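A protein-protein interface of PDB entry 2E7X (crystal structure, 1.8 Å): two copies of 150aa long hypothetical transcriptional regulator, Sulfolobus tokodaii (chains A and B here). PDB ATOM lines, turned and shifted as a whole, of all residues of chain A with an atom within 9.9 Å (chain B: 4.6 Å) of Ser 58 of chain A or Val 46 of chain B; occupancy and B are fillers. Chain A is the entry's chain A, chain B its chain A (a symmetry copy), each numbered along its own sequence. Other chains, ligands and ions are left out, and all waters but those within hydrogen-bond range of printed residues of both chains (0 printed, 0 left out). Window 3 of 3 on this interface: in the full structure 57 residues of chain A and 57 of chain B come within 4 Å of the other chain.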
ATOM      1  N   ALA A  52      32.965  26.476  -9.003  1.00  0.00           N
ATOM      2  CA  ALA A  52      32.864  25.740  -7.758  1.00  0.00           C
ATOM      3  C   ALA A  52      33.120  24.286  -8.150  1.00  0.00           C
ATOM      4  O   ALA A  52      32.555  23.798  -9.130  1.00  0.00           O
ATOM      5  CB  ALA A  52      31.469  25.883  -7.169  1.00  0.00           C
ATOM      6  N   TYR A  53      33.987  23.602  -7.411  1.00  0.00           N
ATOM      7  CA  TYR A  53      34.266  22.202  -7.698  1.00  0.00           C
ATOM      8  C   TYR A  53      33.222  21.375  -6.962  1.00  0.00           C
ATOM      9  O   TYR A  53      33.248  21.269  -5.737  1.00  0.00           O
ATOM     10  CB  TYR A  53      35.678  21.824  -7.235  1.00  0.00           C
ATOM     11  CG  TYR A  53      35.966  20.336  -7.268  1.00  0.00           C
ATOM     12  CD1 TYR A  53      35.695  19.575  -8.404  1.00  0.00           C
ATOM     13  CD2 TYR A  53      36.506  19.689  -6.157  1.00  0.00           C
ATOM     14  CE1 TYR A  53      35.951  18.205  -8.435  1.00  0.00           C
ATOM     15  CE2 TYR A  53      36.768  18.318  -6.173  1.00  0.00           C
ATOM     16  CZ  TYR A  53      36.487  17.582  -7.316  1.00  0.00           C
ATOM     17  OH  TYR A  53      36.733  16.226  -7.336  1.00  0.00           O
ATOM     18  N   ILE A  54      32.290  20.808  -7.720  1.00  0.00           N
ATOM     19  CA  ILE A  54      31.220  20.009  -7.142  1.00  0.00           C
ATOM     20  C   ILE A  54      31.549  18.528  -7.179  1.00  0.00           C
ATOM     21  O   ILE A  54      31.999  18.005  -8.199  1.00  0.00           O
ATOM     22  CB  ILE A  54      29.886  20.256  -7.888  1.00  0.00           C
ATOM     23  CG1 ILE A  54      29.509  21.736  -7.775  1.00  0.00           C
ATOM     24  CG2 ILE A  54      28.783  19.370  -7.314  1.00  0.00           C
ATOM     25  CD1 ILE A  54      28.355  22.150  -8.653  1.00  0.00           C
ATOM     26  N   ASN A  55      31.326  17.862  -6.052  1.00  0.00           N
ATOM     27  CA  ASN A  55      31.582  16.436  -5.931  1.00  0.00           C
ATOM     28  C   ASN A  55      30.573  15.671  -6.786  1.00  0.00           C
ATOM     29  O   ASN A  55      29.386  15.631  -6.473  1.00  0.00           O
ATOM     30  CB  ASN A  55      31.466  16.017  -4.464  1.00  0.00           C
ATOM     31  CG  ASN A  55      31.726  14.539  -4.255  1.00  0.00           C
ATOM     32  OD1 ASN A  55      32.668  13.976  -4.816  1.00  0.00           O
ATOM     33  ND2 ASN A  55      30.900  13.905  -3.434  1.00  0.00           N
ATOM     34  N   PRO A  56      31.039  15.061  -7.887  1.00  0.00           N
ATOM     35  CA  PRO A  56      30.160  14.303  -8.782  1.00  0.00           C
ATOM     36  C   PRO A  56      29.347  13.229  -8.064  1.00  0.00           C
ATOM     37  O   PRO A  56      28.233  12.906  -8.475  1.00  0.00           O
ATOM     38  CB  PRO A  56      31.135  13.711  -9.798  1.00  0.00           C
ATOM     39  CG  PRO A  56      32.209  14.758  -9.870  1.00  0.00           C
ATOM     40  CD  PRO A  56      32.417  15.079  -8.406  1.00  0.00           C
ATOM     41  N   ALA A  57      29.902  12.684  -6.987  1.00  0.00           N
ATOM     42  CA  ALA A  57      29.215  11.647  -6.226  1.00  0.00           C
ATOM     43  C   ALA A  57      27.939  12.178  -5.592  1.00  0.00           C
ATOM     44  O   ALA A  57      26.933  11.471  -5.513  1.00  0.00           O
ATOM     45  CB  ALA A  57      30.142  11.085  -5.153  1.00  0.00           C
ATOM     46  N   SER A  58      27.979  13.429  -5.144  1.00  0.00           N
ATOM     47  CA  SER A  58      26.821  14.052  -4.517  1.00  0.00           C
ATOM     48  C   SER A  58      25.654  14.109  -5.495  1.00  0.00           C
ATOM     49  O   SER A  58      24.494  14.167  -5.090  1.00  0.00           O
ATOM     50  CB  SER A  58      27.174  15.467  -4.053  1.00  0.00           C
ATOM     51  OG  SER A  58      28.293  15.445  -3.183  1.00  0.00           O
ATOM     52  N   LEU A  59      25.970  14.095  -6.787  1.00  0.00           N
ATOM     53  CA  LEU A  59      24.951  14.140  -7.825  1.00  0.00           C
ATOM     54  C   LEU A  59      24.703  12.742  -8.381  1.00  0.00           C
ATOM     55  O   LEU A  59      24.048  12.577  -9.408  1.00  0.00           O
ATOM     56  CB  LEU A  59      25.389  15.083  -8.947  1.00  0.00           C
ATOM     57  CG  LEU A  59      25.517  16.547  -8.515  1.00  0.00           C
ATOM     58  CD1 LEU A  59      26.105  17.376  -9.641  1.00  0.00           C
ATOM     59  CD2 LEU A  59      24.147  17.072  -8.116  1.00  0.00           C
ATOM     60  N   ASN A  60      25.242  11.742  -7.692  1.00  0.00           N
ATOM     61  CA  ASN A  60      25.083  10.346  -8.084  1.00  0.00           C
ATOM     62  C   ASN A  60      25.619  10.022  -9.474  1.00  0.00           C
ATOM     63  O   ASN A  60      25.128   9.104 -10.128  1.00  0.00           O
ATOM     64  CB  ASN A  60      23.609   9.946  -8.005  1.00  0.00           C
ATOM     65  CG  ASN A  60      23.060  10.033  -6.597  1.00  0.00           C
ATOM     66  OD1 ASN A  60      22.092  10.749  -6.339  1.00  0.00           O
ATOM     67  ND2 ASN A  60      23.681   9.307  -5.675  1.00  0.00           N
ATOM     68  N   LEU A  61      26.617  10.773  -9.923  1.00  0.00           N
ATOM     69  CA  LEU A  61      27.211  10.524 -11.232  1.00  0.00           C
ATOM     70  C   LEU A  61      28.196   9.366 -11.068  1.00  0.00           C
ATOM     71  O   LEU A  61      29.403   9.573 -10.938  1.00  0.00           O
ATOM     72  CB  LEU A  61      27.918  11.787 -11.735  1.00  0.00           C
ATOM     73  CG  LEU A  61      26.975  12.965 -12.010  1.00  0.00           C
ATOM     74  CD1 LEU A  61      27.782  14.241 -12.228  1.00  0.00           C
ATOM     75  CD2 LEU A  61      26.101  12.655 -13.229  1.00  0.00           C
ATOM     76  N   ASP A  62      27.662   8.148 -11.063  1.00  0.00           N
ATOM     77  CA  ASP A  62      28.466   6.941 -10.874  1.00  0.00           C
ATOM     78  C   ASP A  62      28.808   6.202 -12.163  1.00  0.00           C
ATOM     79  O   ASP A  62      29.608   5.264 -12.151  1.00  0.00           O
ATOM     80  CB  ASP A  62      27.738   5.980  -9.930  1.00  0.00           C
ATOM     81  CG  ASP A  62      27.439   6.605  -8.583  1.00  0.00           C
ATOM     82  OD1 ASP A  62      28.383   7.130  -7.954  1.00  0.00           O
ATOM     83  OD2 ASP A  62      26.263   6.568  -8.154  1.00  0.00           O
ATOM     84  N   ARG A 108      29.715  11.782 -18.050  1.00  0.00           N
ATOM     85  CA  ARG A 108      29.265  11.300 -16.746  1.00  0.00           C
ATOM     86  C   ARG A 108      27.747  11.161 -16.745  1.00  0.00           C
ATOM     87  O   ARG A 108      27.048  12.018 -17.283  1.00  0.00           O
ATOM     88  CB  ARG A 108      29.618  12.295 -15.632  1.00  0.00           C
ATOM     89  CG  ARG A 108      31.020  12.873 -15.618  1.00  0.00           C
ATOM     90  CD  ARG A 108      31.217  13.626 -14.298  1.00  0.00           C
ATOM     91  NE  ARG A 108      32.515  14.283 -14.178  1.00  0.00           N
ATOM     92  CZ  ARG A 108      32.745  15.560 -14.469  1.00  0.00           C
ATOM     93  NH1 ARG A 108      31.761  16.338 -14.903  1.00  0.00           N
ATOM     94  NH2 ARG A 108      33.963  16.062 -14.321  1.00  0.00           N
ATOM     95  N   LYS A 110      24.279   9.179 -14.255  1.00  0.00           N
ATOM     96  CA  LYS A 110      23.908   8.578 -12.981  1.00  0.00           C
ATOM     97  C   LYS A 110      23.779   7.066 -13.085  1.00  0.00           C
ATOM     98  O   LYS A 110      24.136   6.344 -12.157  1.00  0.00           O
ATOM     99  CB  LYS A 110      22.576   9.147 -12.491  1.00  0.00           C
ATOM    100  CG  LYS A 110      22.580  10.638 -12.230  1.00  0.00           C
ATOM    101  CD  LYS A 110      21.204  11.111 -11.782  1.00  0.00           C
ATOM    102  CE  LYS A 110      20.146  10.813 -12.841  1.00  0.00           C
ATOM    103  NZ  LYS A 110      18.778  11.167 -12.377  1.00  0.00           N
ATOM    104  N   MET B   1      20.080  17.475  -0.188  1.00  0.00           N
ATOM    105  CA  MET B   1      19.867  18.443  -1.302  1.00  0.00           C
ATOM    106  C   MET B   1      18.440  18.402  -1.824  1.00  0.00           C
ATOM    107  O   MET B   1      17.738  17.402  -1.672  1.00  0.00           O
ATOM    108  CB  MET B   1      20.808  18.134  -2.467  1.00  0.00           C
ATOM    109  CG  MET B   1      22.248  18.563  -2.276  1.00  0.00           C
ATOM    110  SD  MET B   1      23.241  18.051  -3.690  1.00  0.00           S
ATOM    111  CE  MET B   1      22.327  18.772  -5.010  1.00  0.00           C
ATOM    112  N   LEU B   9      23.724  25.256  -7.364  1.00  0.00           N
ATOM    113  CA  LEU B   9      24.903  24.586  -7.900  1.00  0.00           C
ATOM    114  C   LEU B   9      25.040  24.795  -9.411  1.00  0.00           C
ATOM    115  O   LEU B   9      26.151  24.923  -9.929  1.00  0.00           O
ATOM    116  CB  LEU B   9      24.848  23.083  -7.591  1.00  0.00           C
ATOM    117  CG  LEU B   9      24.971  22.675  -6.120  1.00  0.00           C
ATOM    118  CD1 LEU B   9      24.860  21.163  -5.999  1.00  0.00           C
ATOM    119  CD2 LEU B   9      26.304  23.156  -5.559  1.00  0.00           C
ATOM    120  N   LEU B  41      26.192  23.148   1.864  1.00  0.00           N
ATOM    121  CA  LEU B  41      26.688  22.359   0.739  1.00  0.00           C
ATOM    122  C   LEU B  41      28.196  22.179   0.855  1.00  0.00           C
ATOM    123  O   LEU B  41      28.736  21.131   0.492  1.00  0.00           O
ATOM    124  CB  LEU B  41      26.344  23.049  -0.584  1.00  0.00           C
ATOM    125  CG  LEU B  41      24.859  23.046  -0.952  1.00  0.00           C
ATOM    126  CD1 LEU B  41      24.605  24.029  -2.085  1.00  0.00           C
ATOM    127  CD2 LEU B  41      24.435  21.637  -1.349  1.00  0.00           C
ATOM    128  N   ASP B  44      28.767  19.800   3.910  1.00  0.00           N
ATOM    129  CA  ASP B  44      28.425  18.420   3.579  1.00  0.00           C
ATOM    130  C   ASP B  44      29.318  17.805   2.507  1.00  0.00           C
ATOM    131  O   ASP B  44      29.136  16.645   2.136  1.00  0.00           O
ATOM    132  CB  ASP B  44      26.963  18.314   3.134  1.00  0.00           C
ATOM    133  CG  ASP B  44      25.989  18.624   4.254  1.00  0.00           C
ATOM    134  OD1 ASP B  44      26.421  18.670   5.426  1.00  0.00           O
ATOM    135  OD2 ASP B  44      24.788  18.811   3.962  1.00  0.00           O
ATOM    136  N   GLY B  45      30.270  18.582   2.003  1.00  0.00           N
ATOM    137  CA  GLY B  45      31.179  18.072   0.990  1.00  0.00           C
ATOM    138  C   GLY B  45      30.679  18.065  -0.444  1.00  0.00           C
ATOM    139  O   GLY B  45      31.346  17.514  -1.321  1.00  0.00           O
ATOM    140  N   VAL B  46      29.514  18.657  -0.694  1.00  0.00           N
ATOM    141  CA  VAL B  46      28.975  18.711  -2.054  1.00  0.00           C
ATOM    142  C   VAL B  46      29.845  19.680  -2.849  1.00  0.00           C
ATOM    143  O   VAL B  46      30.240  19.405  -3.986  1.00  0.00           O
ATOM    144  CB  VAL B  46      27.510  19.192  -2.053  1.00  0.00           C
ATOM    145  CG1 VAL B  46      26.980  19.271  -3.486  1.00  0.00           C
ATOM    146  CG2 VAL B  46      26.661  18.238  -1.225  1.00  0.00           C
ATOM    147  N   ILE B  47      30.131  20.828  -2.243  1.00  0.00           N
ATOM    148  CA  ILE B  47      31.005  21.817  -2.854  1.00  0.00           C
ATOM    149  C   ILE B  47      32.340  21.567  -2.162  1.00  0.00           C
ATOM    150  O   ILE B  47      32.483  21.837  -0.972  1.00  0.00           O
ATOM    151  CB  ILE B  47      30.540  23.262  -2.560  1.00  0.00           C
ATOM    152  CG1 ILE B  47      29.206  23.531  -3.263  1.00  0.00           C
ATOM    153  CG2 ILE B  47      31.600  24.249  -3.011  1.00  0.00           C
ATOM    154  CD1 ILE B  47      28.632  24.922  -2.992  1.00  0.00           C
ATOM    155  N   LYS B  48      33.306  21.033  -2.901  1.00  0.00           N
ATOM    156  CA  LYS B  48      34.610  20.722  -2.326  1.00  0.00           C
ATOM    157  C   LYS B  48      35.599  21.875  -2.396  1.00  0.00           C
ATOM    158  O   LYS B  48      36.649  21.845  -1.748  1.00  0.00           O
ATOM    159  CB  LYS B  48      35.196  19.492  -3.017  1.00  0.00           C
ATOM    160  CG  LYS B  48      34.259  18.293  -3.004  1.00  0.00           C
ATOM    161  CD  LYS B  48      34.959  17.020  -3.451  1.00  0.00           C
ATOM    162  CE  LYS B  48      36.037  16.613  -2.458  1.00  0.00           C
ATOM    163  NZ  LYS B  48      36.682  15.327  -2.838  1.00  0.00           N
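The side-chain amide nitrogen (ND2) of Asn 55 of chain A lies within hydrogen-bond range of the side-chain hydroxyl (OG) of Ser 58 of chain A (3.0 Å).
O of Leu 41 of chain B is in hydrogen-bond range of N of Val 46 of chain B (2.9 Å).
O of Leu 41 of chain B lies within hydrogen-bond range of N of Ile 47 of chain B.
Printed residues of chain B within 4 Å of Tyr 53 of chain A: Val 46 (3.9 Å), Ile 47 (3.7 Å) and Lys 48 (2.8 Å).
Of the printed residues of chain A, Met 1 of chain B touches Leu 59.
No residue of chain A comes within 4 Å of Leu 41 of chain B.
Of chain A, only Asn 55 comes within 4 Å of Gly 45 of chain B.
Of chain A, only Tyr 53 (3.9 Å), Ile 54 (3.4 Å), Asn 55 (2.8 Å) and Ser 58 (3.5 Å) come within 4 Å of Val 46 of chain B.
The nearest residue of chain A that does not touch Val 46 of chain B is Leu 59 of chain A (5.9 Å).
N of Lys 48 of chain B is in hydrogen-bond range of O of Tyr 53 of chain A (2.8 Å).
The backbone carbonyl oxygen (O) of Val 46 of chain B is in hydrogen-bond range of the backbone NH (N) of Asn 55 of chain A (2.8 Å).
O of Tyr 53 of chain A touches O of Val 46 of chain B, at 3.9 Å.
Ile 47 of chain B touches Tyr 53 of chain A (CA to O, 3.7 Å).
Ile 54 of chain A touches Leu 9 of chain B.
Val 46 of chain B touches Ile 54 of chain A.
O of Gly 45 of chain B touches CB of Asn 55 of chain A, 3.5 Å away.
Lys 48 of chain B touches Asn 55 of chain A (CD to CB, 3.8 Å).
OG of Ser 58 of chain A touches CA of Val 46 of chain B, 3.5 Å away.
Leu 59 of chain A touches Met 1 of chain B (CD2 to CE, 3.98 Å).
Of the 8 printed residues of chain B, 6 touch a printed residue of chain A.
Printed residues of chain B that touch a printed residue of chain A: Met 1, Leu 9, Gly 45, Val 46, Ile 47 and Lys 48.
Hydrophobic or aromatic side chains of chain B within 4 Å of the printed part of chain A: Met 1, Leu 9 and Val 46.
Along chain B the printed residues that touch a printed residue of chain A span positions 1 to 48.
Hydrophobic or aromatic side chains of chain A that line the printed part of chain B: Tyr 53, Ile 54 and Leu 59.
Along chain A the printed residues that touch a printed residue of chain B span positions 53 to 59.
Among the printed residues, no Asp or Glu carboxylate lies within 4 Å of a Lys or Arg side-chain nitrogen of the other chain.
No position is printed for both chains.
Of the 10 pairs that touch across the chains among the printed residues, none has its exchanged pair printed and touching as well.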
